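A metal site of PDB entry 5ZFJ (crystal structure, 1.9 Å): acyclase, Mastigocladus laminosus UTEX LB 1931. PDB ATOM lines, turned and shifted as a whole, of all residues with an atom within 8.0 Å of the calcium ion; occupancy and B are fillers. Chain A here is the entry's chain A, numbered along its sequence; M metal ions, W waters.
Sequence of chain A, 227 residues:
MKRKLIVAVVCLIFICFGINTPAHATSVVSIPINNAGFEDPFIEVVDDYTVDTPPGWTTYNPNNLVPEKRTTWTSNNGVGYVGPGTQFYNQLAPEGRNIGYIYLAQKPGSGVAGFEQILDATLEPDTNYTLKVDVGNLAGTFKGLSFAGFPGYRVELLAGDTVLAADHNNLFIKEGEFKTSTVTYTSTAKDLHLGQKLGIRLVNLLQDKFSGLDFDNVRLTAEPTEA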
ATOM      1  N   PHE A  88       6.071 -13.469 -28.330  1.00  0.00           N
ATOM      2  CA  PHE A  88       5.412 -12.555 -27.375  1.00  0.00           C
ATOM      3  C   PHE A  88       4.875 -11.240 -27.973  1.00  0.00           C
ATOM      4  O   PHE A  88       4.007 -10.616 -27.369  1.00  0.00           O
ATOM      5  CB  PHE A  88       6.410 -12.196 -26.276  1.00  0.00           C
ATOM      6  CG  PHE A  88       6.680 -13.348 -25.337  1.00  0.00           C
ATOM      7  CD1 PHE A  88       5.637 -14.119 -24.851  1.00  0.00           C
ATOM      8  CD2 PHE A  88       7.982 -13.649 -24.941  1.00  0.00           C
ATOM      9  CE1 PHE A  88       5.879 -15.152 -23.973  1.00  0.00           C
ATOM     10  CE2 PHE A  88       8.217 -14.693 -24.067  1.00  0.00           C
ATOM     11  CZ  PHE A  88       7.168 -15.435 -23.576  1.00  0.00           C
ATOM     12  N   TYR A  89       5.461 -10.809 -29.104  1.00  0.00           N
ATOM     13  CA  TYR A  89       5.260  -9.504 -29.665  1.00  0.00           C
ATOM     14  C   TYR A  89       5.214  -9.609 -31.193  1.00  0.00           C
ATOM     15  O   TYR A  89       5.794 -10.524 -31.778  1.00  0.00           O
ATOM     16  CB  TYR A  89       6.380  -8.560 -29.247  1.00  0.00           C
ATOM     17  CG  TYR A  89       6.285  -8.116 -27.806  1.00  0.00           C
ATOM     18  CD1 TYR A  89       5.349  -7.166 -27.422  1.00  0.00           C
ATOM     19  CD2 TYR A  89       7.108  -8.652 -26.830  1.00  0.00           C
ATOM     20  CE1 TYR A  89       5.251  -6.730 -26.108  1.00  0.00           C
ATOM     21  CE2 TYR A  89       6.996  -8.275 -25.499  1.00  0.00           C
ATOM     22  CZ  TYR A  89       6.081  -7.293 -25.147  1.00  0.00           C
ATOM     23  OH  TYR A  89       6.003  -6.869 -23.863  1.00  0.00           O
ATOM     24  N   GLY A 136       5.454  -2.291 -22.854  1.00  0.00           N
ATOM     25  CA  GLY A 136       5.052  -3.430 -23.664  1.00  0.00           C
ATOM     26  C   GLY A 136       3.972  -4.260 -23.011  1.00  0.00           C
ATOM     27  O   GLY A 136       4.032  -4.510 -21.797  1.00  0.00           O
ATOM     28  N   ASN A 137       3.024  -4.721 -23.832  1.00  0.00           N
ATOM     29  CA  ASN A 137       1.932  -5.603 -23.421  1.00  0.00           C
ATOM     30  C   ASN A 137       2.194  -6.921 -24.141  1.00  0.00           C
ATOM     31  O   ASN A 137       2.032  -7.044 -25.360  1.00  0.00           O
ATOM     32  CB  ASN A 137       0.576  -4.966 -23.732  1.00  0.00           C
ATOM     33  CG  ASN A 137      -0.605  -5.870 -23.466  1.00  0.00           C
ATOM     34  OD1 ASN A 137      -0.447  -6.964 -22.919  1.00  0.00           O
ATOM     35  ND2 ASN A 137      -1.796  -5.393 -23.793  1.00  0.00           N
ATOM     36  N   LEU A 138       2.656  -7.890 -23.366  1.00  0.00           N
ATOM     37  CA  LEU A 138       3.091  -9.187 -23.894  1.00  0.00           C
ATOM     38  C   LEU A 138       1.851  -9.983 -24.353  1.00  0.00           C
ATOM     39  O   LEU A 138       0.797  -9.878 -23.729  1.00  0.00           O
ATOM     40  CB  LEU A 138       3.816  -9.870 -22.739  1.00  0.00           C
ATOM     41  CG  LEU A 138       4.659 -11.091 -23.053  1.00  0.00           C
ATOM     42  CD1 LEU A 138       6.121 -10.760 -22.979  1.00  0.00           C
ATOM     43  CD2 LEU A 138       4.315 -12.183 -22.055  1.00  0.00           C
ATOM     44  N   ALA A 139       1.962 -10.677 -25.483  1.00  0.00           N
ATOM     45  CA  ALA A 139       0.855 -11.388 -26.138  1.00  0.00           C
ATOM     46  C   ALA A 139       1.137 -12.887 -26.187  1.00  0.00           C
ATOM     47  O   ALA A 139       2.283 -13.302 -26.083  1.00  0.00           O
ATOM     48  CB  ALA A 139       0.669 -10.880 -27.546  1.00  0.00           C
ATOM     49  N   GLY A 140       0.096 -13.684 -26.413  1.00  0.00           N
ATOM     50  CA  GLY A 140       0.222 -15.098 -26.763  1.00  0.00           C
ATOM     51  C   GLY A 140      -0.218 -16.052 -25.668  1.00  0.00           C
ATOM     52  O   GLY A 140      -0.902 -15.685 -24.702  1.00  0.00           O
ATOM     53  N   SER A 146      -1.816 -18.178 -20.361  1.00  0.00           N
ATOM     54  CA  SER A 146      -2.344 -17.111 -21.241  1.00  0.00           C
ATOM     55  C   SER A 146      -1.686 -15.769 -20.912  1.00  0.00           C
ATOM     56  O   SER A 146      -1.656 -15.405 -19.746  1.00  0.00           O
ATOM     57  CB  SER A 146      -3.831 -16.983 -21.126  1.00  0.00           C
ATOM     58  OG  SER A 146      -4.299 -15.965 -22.005  1.00  0.00           O
ATOM     59  N   PHE A 147      -1.196 -15.038 -21.922  1.00  0.00           N
ATOM     60  CA  PHE A 147      -0.625 -13.714 -21.706  1.00  0.00           C
ATOM     61  C   PHE A 147      -1.612 -12.606 -22.077  1.00  0.00           C
ATOM     62  O   PHE A 147      -1.272 -11.427 -22.017  1.00  0.00           O
ATOM     63  CB  PHE A 147       0.712 -13.613 -22.453  1.00  0.00           C
ATOM     64  CG  PHE A 147       1.633 -14.742 -22.098  1.00  0.00           C
ATOM     65  CD1 PHE A 147       1.955 -15.019 -20.781  1.00  0.00           C
ATOM     66  CD2 PHE A 147       2.112 -15.595 -23.083  1.00  0.00           C
ATOM     67  CE1 PHE A 147       2.784 -16.070 -20.447  1.00  0.00           C
ATOM     68  CE2 PHE A 147       2.954 -16.654 -22.748  1.00  0.00           C
ATOM     69  CZ  PHE A 147       3.271 -16.900 -21.435  1.00  0.00           C
ATOM     70  N   ALA A 148      -2.852 -12.948 -22.405  1.00  0.00           N
ATOM     71  CA  ALA A 148      -3.881 -11.934 -22.648  1.00  0.00           C
ATOM     72  C   ALA A 148      -4.037 -11.062 -21.404  1.00  0.00           C
ATOM     73  O   ALA A 148      -4.014 -11.556 -20.261  1.00  0.00           O
ATOM     74  CB  ALA A 148      -5.178 -12.619 -22.978  1.00  0.00           C
ATOM     75  N   GLY A 149      -4.301  -9.771 -21.616  1.00  0.00           N
ATOM     76  CA  GLY A 149      -4.578  -8.870 -20.501  1.00  0.00           C
ATOM     77  C   GLY A 149      -3.326  -8.121 -20.113  1.00  0.00           C
ATOM     78  O   GLY A 149      -2.227  -8.417 -20.604  1.00  0.00           O
ATOM     79  N   PHE A 150      -3.462  -7.125 -19.244  1.00  0.00           N
ATOM     80  CA  PHE A 150      -2.384  -6.176 -19.019  1.00  0.00           C
ATOM     81  C   PHE A 150      -2.586  -5.601 -17.620  1.00  0.00           C
ATOM     82  O   PHE A 150      -3.717  -5.333 -17.244  1.00  0.00           O
ATOM     83  CB  PHE A 150      -2.408  -5.109 -20.120  1.00  0.00           C
ATOM     84  CG  PHE A 150      -1.328  -4.074 -20.022  1.00  0.00           C
ATOM     85  CD1 PHE A 150      -0.032  -4.388 -20.358  1.00  0.00           C
ATOM     86  CD2 PHE A 150      -1.592  -2.793 -19.550  1.00  0.00           C
ATOM     87  CE1 PHE A 150       0.964  -3.427 -20.291  1.00  0.00           C
ATOM     88  CE2 PHE A 150      -0.596  -1.832 -19.483  1.00  0.00           C
ATOM     89  CZ  PHE A 150       0.686  -2.155 -19.844  1.00  0.00           C
ATOM     90  N   PRO A 151      -1.517  -5.438 -16.790  1.00  0.00           N
ATOM     91  CA  PRO A 151      -1.702  -5.013 -15.400  1.00  0.00           C
ATOM     92  C   PRO A 151      -1.830  -3.507 -15.156  1.00  0.00           C
ATOM     93  O   PRO A 151      -2.106  -3.114 -14.038  1.00  0.00           O
ATOM     94  CB  PRO A 151      -0.432  -5.522 -14.692  1.00  0.00           C
ATOM     95  CG  PRO A 151       0.605  -5.607 -15.782  1.00  0.00           C
ATOM     96  CD  PRO A 151      -0.158  -5.907 -17.055  1.00  0.00           C
ATOM     97  N   ILE A 173      -2.269   0.162 -24.761  1.00  0.00           N
ATOM     98  CA  ILE A 173      -1.220  -0.672 -25.369  1.00  0.00           C
ATOM     99  C   ILE A 173      -1.809  -2.016 -25.779  1.00  0.00           C
ATOM    100  O   ILE A 173      -2.276  -2.798 -24.974  1.00  0.00           O
ATOM    101  CB  ILE A 173      -0.023  -0.854 -24.435  1.00  0.00           C
ATOM    102  CG1 ILE A 173       0.336   0.501 -23.835  1.00  0.00           C
ATOM    103  CG2 ILE A 173       1.127  -1.532 -25.157  1.00  0.00           C
ATOM    104  CD1 ILE A 173       1.521   0.476 -22.922  1.00  0.00           C
ATOM    105  N   LYS A 174      -1.852  -2.220 -27.099  1.00  0.00           N
ATOM    106  CA  LYS A 174      -2.451  -3.435 -27.660  1.00  0.00           C
ATOM    107  C   LYS A 174      -1.560  -4.621 -27.313  1.00  0.00           C
ATOM    108  O   LYS A 174      -0.340  -4.490 -27.159  1.00  0.00           O
ATOM    109  CB  LYS A 174      -2.567  -3.305 -29.190  1.00  0.00           C
ATOM    110  CG  LYS A 174      -3.660  -2.367 -29.659  1.00  0.00           C
ATOM    111  CD  LYS A 174      -3.300  -1.598 -30.912  1.00  0.00           C
ATOM    112  CE  LYS A 174      -2.901  -2.486 -32.074  1.00  0.00           C
ATOM    113  NZ  LYS A 174      -3.868  -2.389 -33.193  1.00  0.00           N
ATOM    114  N   GLU A 175      -2.195  -5.801 -27.249  1.00  0.00           N
ATOM    115  CA  GLU A 175      -1.509  -7.064 -26.997  1.00  0.00           C
ATOM    116  C   GLU A 175      -0.403  -7.211 -28.068  1.00  0.00           C
ATOM    117  O   GLU A 175      -0.679  -7.073 -29.251  1.00  0.00           O
ATOM    118  CB  GLU A 175      -2.491  -8.241 -27.057  1.00  0.00           C
ATOM    119  CG  GLU A 175      -3.418  -8.353 -25.844  1.00  0.00           C
ATOM    120  CD  GLU A 175      -2.784  -8.863 -24.543  1.00  0.00           C
ATOM    121  OE1 GLU A 175      -1.872  -9.699 -24.615  1.00  0.00           O
ATOM    122  OE2 GLU A 175      -3.094  -8.382 -23.433  1.00  0.00           O
ATOM    123  N   GLY A 176       0.844  -7.403 -27.647  1.00  0.00           N
ATOM    124  CA  GLY A 176       1.936  -7.639 -28.584  1.00  0.00           C
ATOM    125  C   GLY A 176       2.584  -6.400 -29.184  1.00  0.00           C
ATOM    126  O   GLY A 176       3.325  -6.524 -30.170  1.00  0.00           O
ATOM    127  N   LYS A 209      -4.788  -9.008 -14.905  1.00  0.00           N
ATOM    128  CA  LYS A 209      -3.961 -10.133 -15.367  1.00  0.00           C
ATOM    129  C   LYS A 209      -4.213 -10.297 -16.861  1.00  0.00           C
ATOM    130  O   LYS A 209      -5.258  -9.864 -17.349  1.00  0.00           O
ATOM    131  CB  LYS A 209      -4.353 -11.419 -14.617  1.00  0.00           C
ATOM    132  CG  LYS A 209      -4.367 -11.252 -13.097  1.00  0.00           C
ATOM    133  CD  LYS A 209      -3.472 -12.189 -12.290  1.00  0.00           C
ATOM    134  CE  LYS A 209      -2.734 -11.520 -11.138  1.00  0.00           C
ATOM    135  NZ  LYS A 209      -1.426 -12.181 -10.924  1.00  0.00           N
ATOM    136  N   PHE A 210      -3.289 -10.882 -17.614  1.00  0.00           N
ATOM    137  CA  PHE A 210      -1.949 -11.289 -17.214  1.00  0.00           C
ATOM    138  C   PHE A 210      -1.103 -10.139 -16.644  1.00  0.00           C
ATOM    139  O   PHE A 210      -0.962  -9.075 -17.259  1.00  0.00           O
ATOM    140  CB  PHE A 210      -1.254 -11.841 -18.467  1.00  0.00           C
ATOM    141  CG  PHE A 210       0.186 -12.235 -18.254  1.00  0.00           C
ATOM    142  CD1 PHE A 210       0.492 -13.396 -17.570  1.00  0.00           C
ATOM    143  CD2 PHE A 210       1.222 -11.437 -18.725  1.00  0.00           C
ATOM    144  CE1 PHE A 210       1.806 -13.788 -17.400  1.00  0.00           C
ATOM    145  CE2 PHE A 210       2.533 -11.834 -18.536  1.00  0.00           C
ATOM    146  CZ  PHE A 210       2.827 -12.986 -17.852  1.00  0.00           C
ATOM    147  N   SER A 211      -0.479 -10.357 -15.478  1.00  0.00           N
ATOM    148  CA  SER A 211       0.127  -9.224 -14.747  1.00  0.00           C
ATOM    149  C   SER A 211       1.653  -9.185 -14.881  1.00  0.00           C
ATOM    150  O   SER A 211       2.391  -9.010 -13.921  1.00  0.00           O
ATOM    151  CB  SER A 211      -0.325  -9.186 -13.303  1.00  0.00           C
ATOM    152  OG  SER A 211      -0.316 -10.484 -12.775  1.00  0.00           O
ATOM    153  N   GLY A 212       2.126  -9.297 -16.120  1.00  0.00           N
ATOM    154  CA  GLY A 212       3.496  -9.019 -16.489  1.00  0.00           C
ATOM    155  C   GLY A 212       3.503  -7.840 -17.435  1.00  0.00           C
ATOM    156  O   GLY A 212       2.529  -7.624 -18.134  1.00  0.00           O
ATOM    157  N   LEU A 213       4.540  -7.005 -17.368  1.00  0.00           N
ATOM    158  CA  LEU A 213       4.722  -5.999 -18.414  1.00  0.00           C
ATOM    159  C   LEU A 213       6.191  -5.655 -18.522  1.00  0.00           C
ATOM    160  O   LEU A 213       6.985  -5.937 -17.611  1.00  0.00           O
ATOM    161  CB  LEU A 213       3.889  -4.733 -18.224  1.00  0.00           C
ATOM    162  CG  LEU A 213       3.991  -3.945 -16.910  1.00  0.00           C
ATOM    163  CD1 LEU A 213       5.135  -4.330 -16.000  1.00  0.00           C
ATOM    164  CD2 LEU A 213       4.045  -2.458 -17.209  1.00  0.00           C
HETATM  165 CA    CA M   1      -0.987  -9.161 -22.457  1.00  0.00          CA
HETATM  166  O   HOH W   1       0.514  -8.543 -20.671  1.00  0.00           O
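Ala 148 touches the calcium ion (C to CA, 3.7 Å). The nearest printed residue that does not touch the calcium ion is Ala 139 (4.5 Å).
The calcium ion is bound by O of Leu 138 (2.3 Å), OD1 of Asn 137 (2.3 Å), O of Phe 147 (2.3 Å), O of Gly 149 (2.4 Å), OE1 of Glu 175 (2.4 Å), water W1 (2.4 Å) and OE2 of Glu 175 (2.4 Å). The calcium ion has seven donor atoms within binding distance.
The backbone NH (N) of Gly 176 is in hydrogen-bond range of the backbone carbonyl oxygen (O) of Asn 137, at 2.6 Å. The side-chain amide nitrogen of Asn 137 sits at hydrogen-bond distance from the backbone carbonyl oxygen of Ile 173. O of Gly 140 sits at hydrogen-bond distance from N of Phe 147, at 2.9 Å. N of Phe 210 lies within hydrogen-bond range of O of Ala 148, 2.8 Å away. N of Ala 148 is in hydrogen-bond range of OG of Ser 146, 3.4 Å away.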
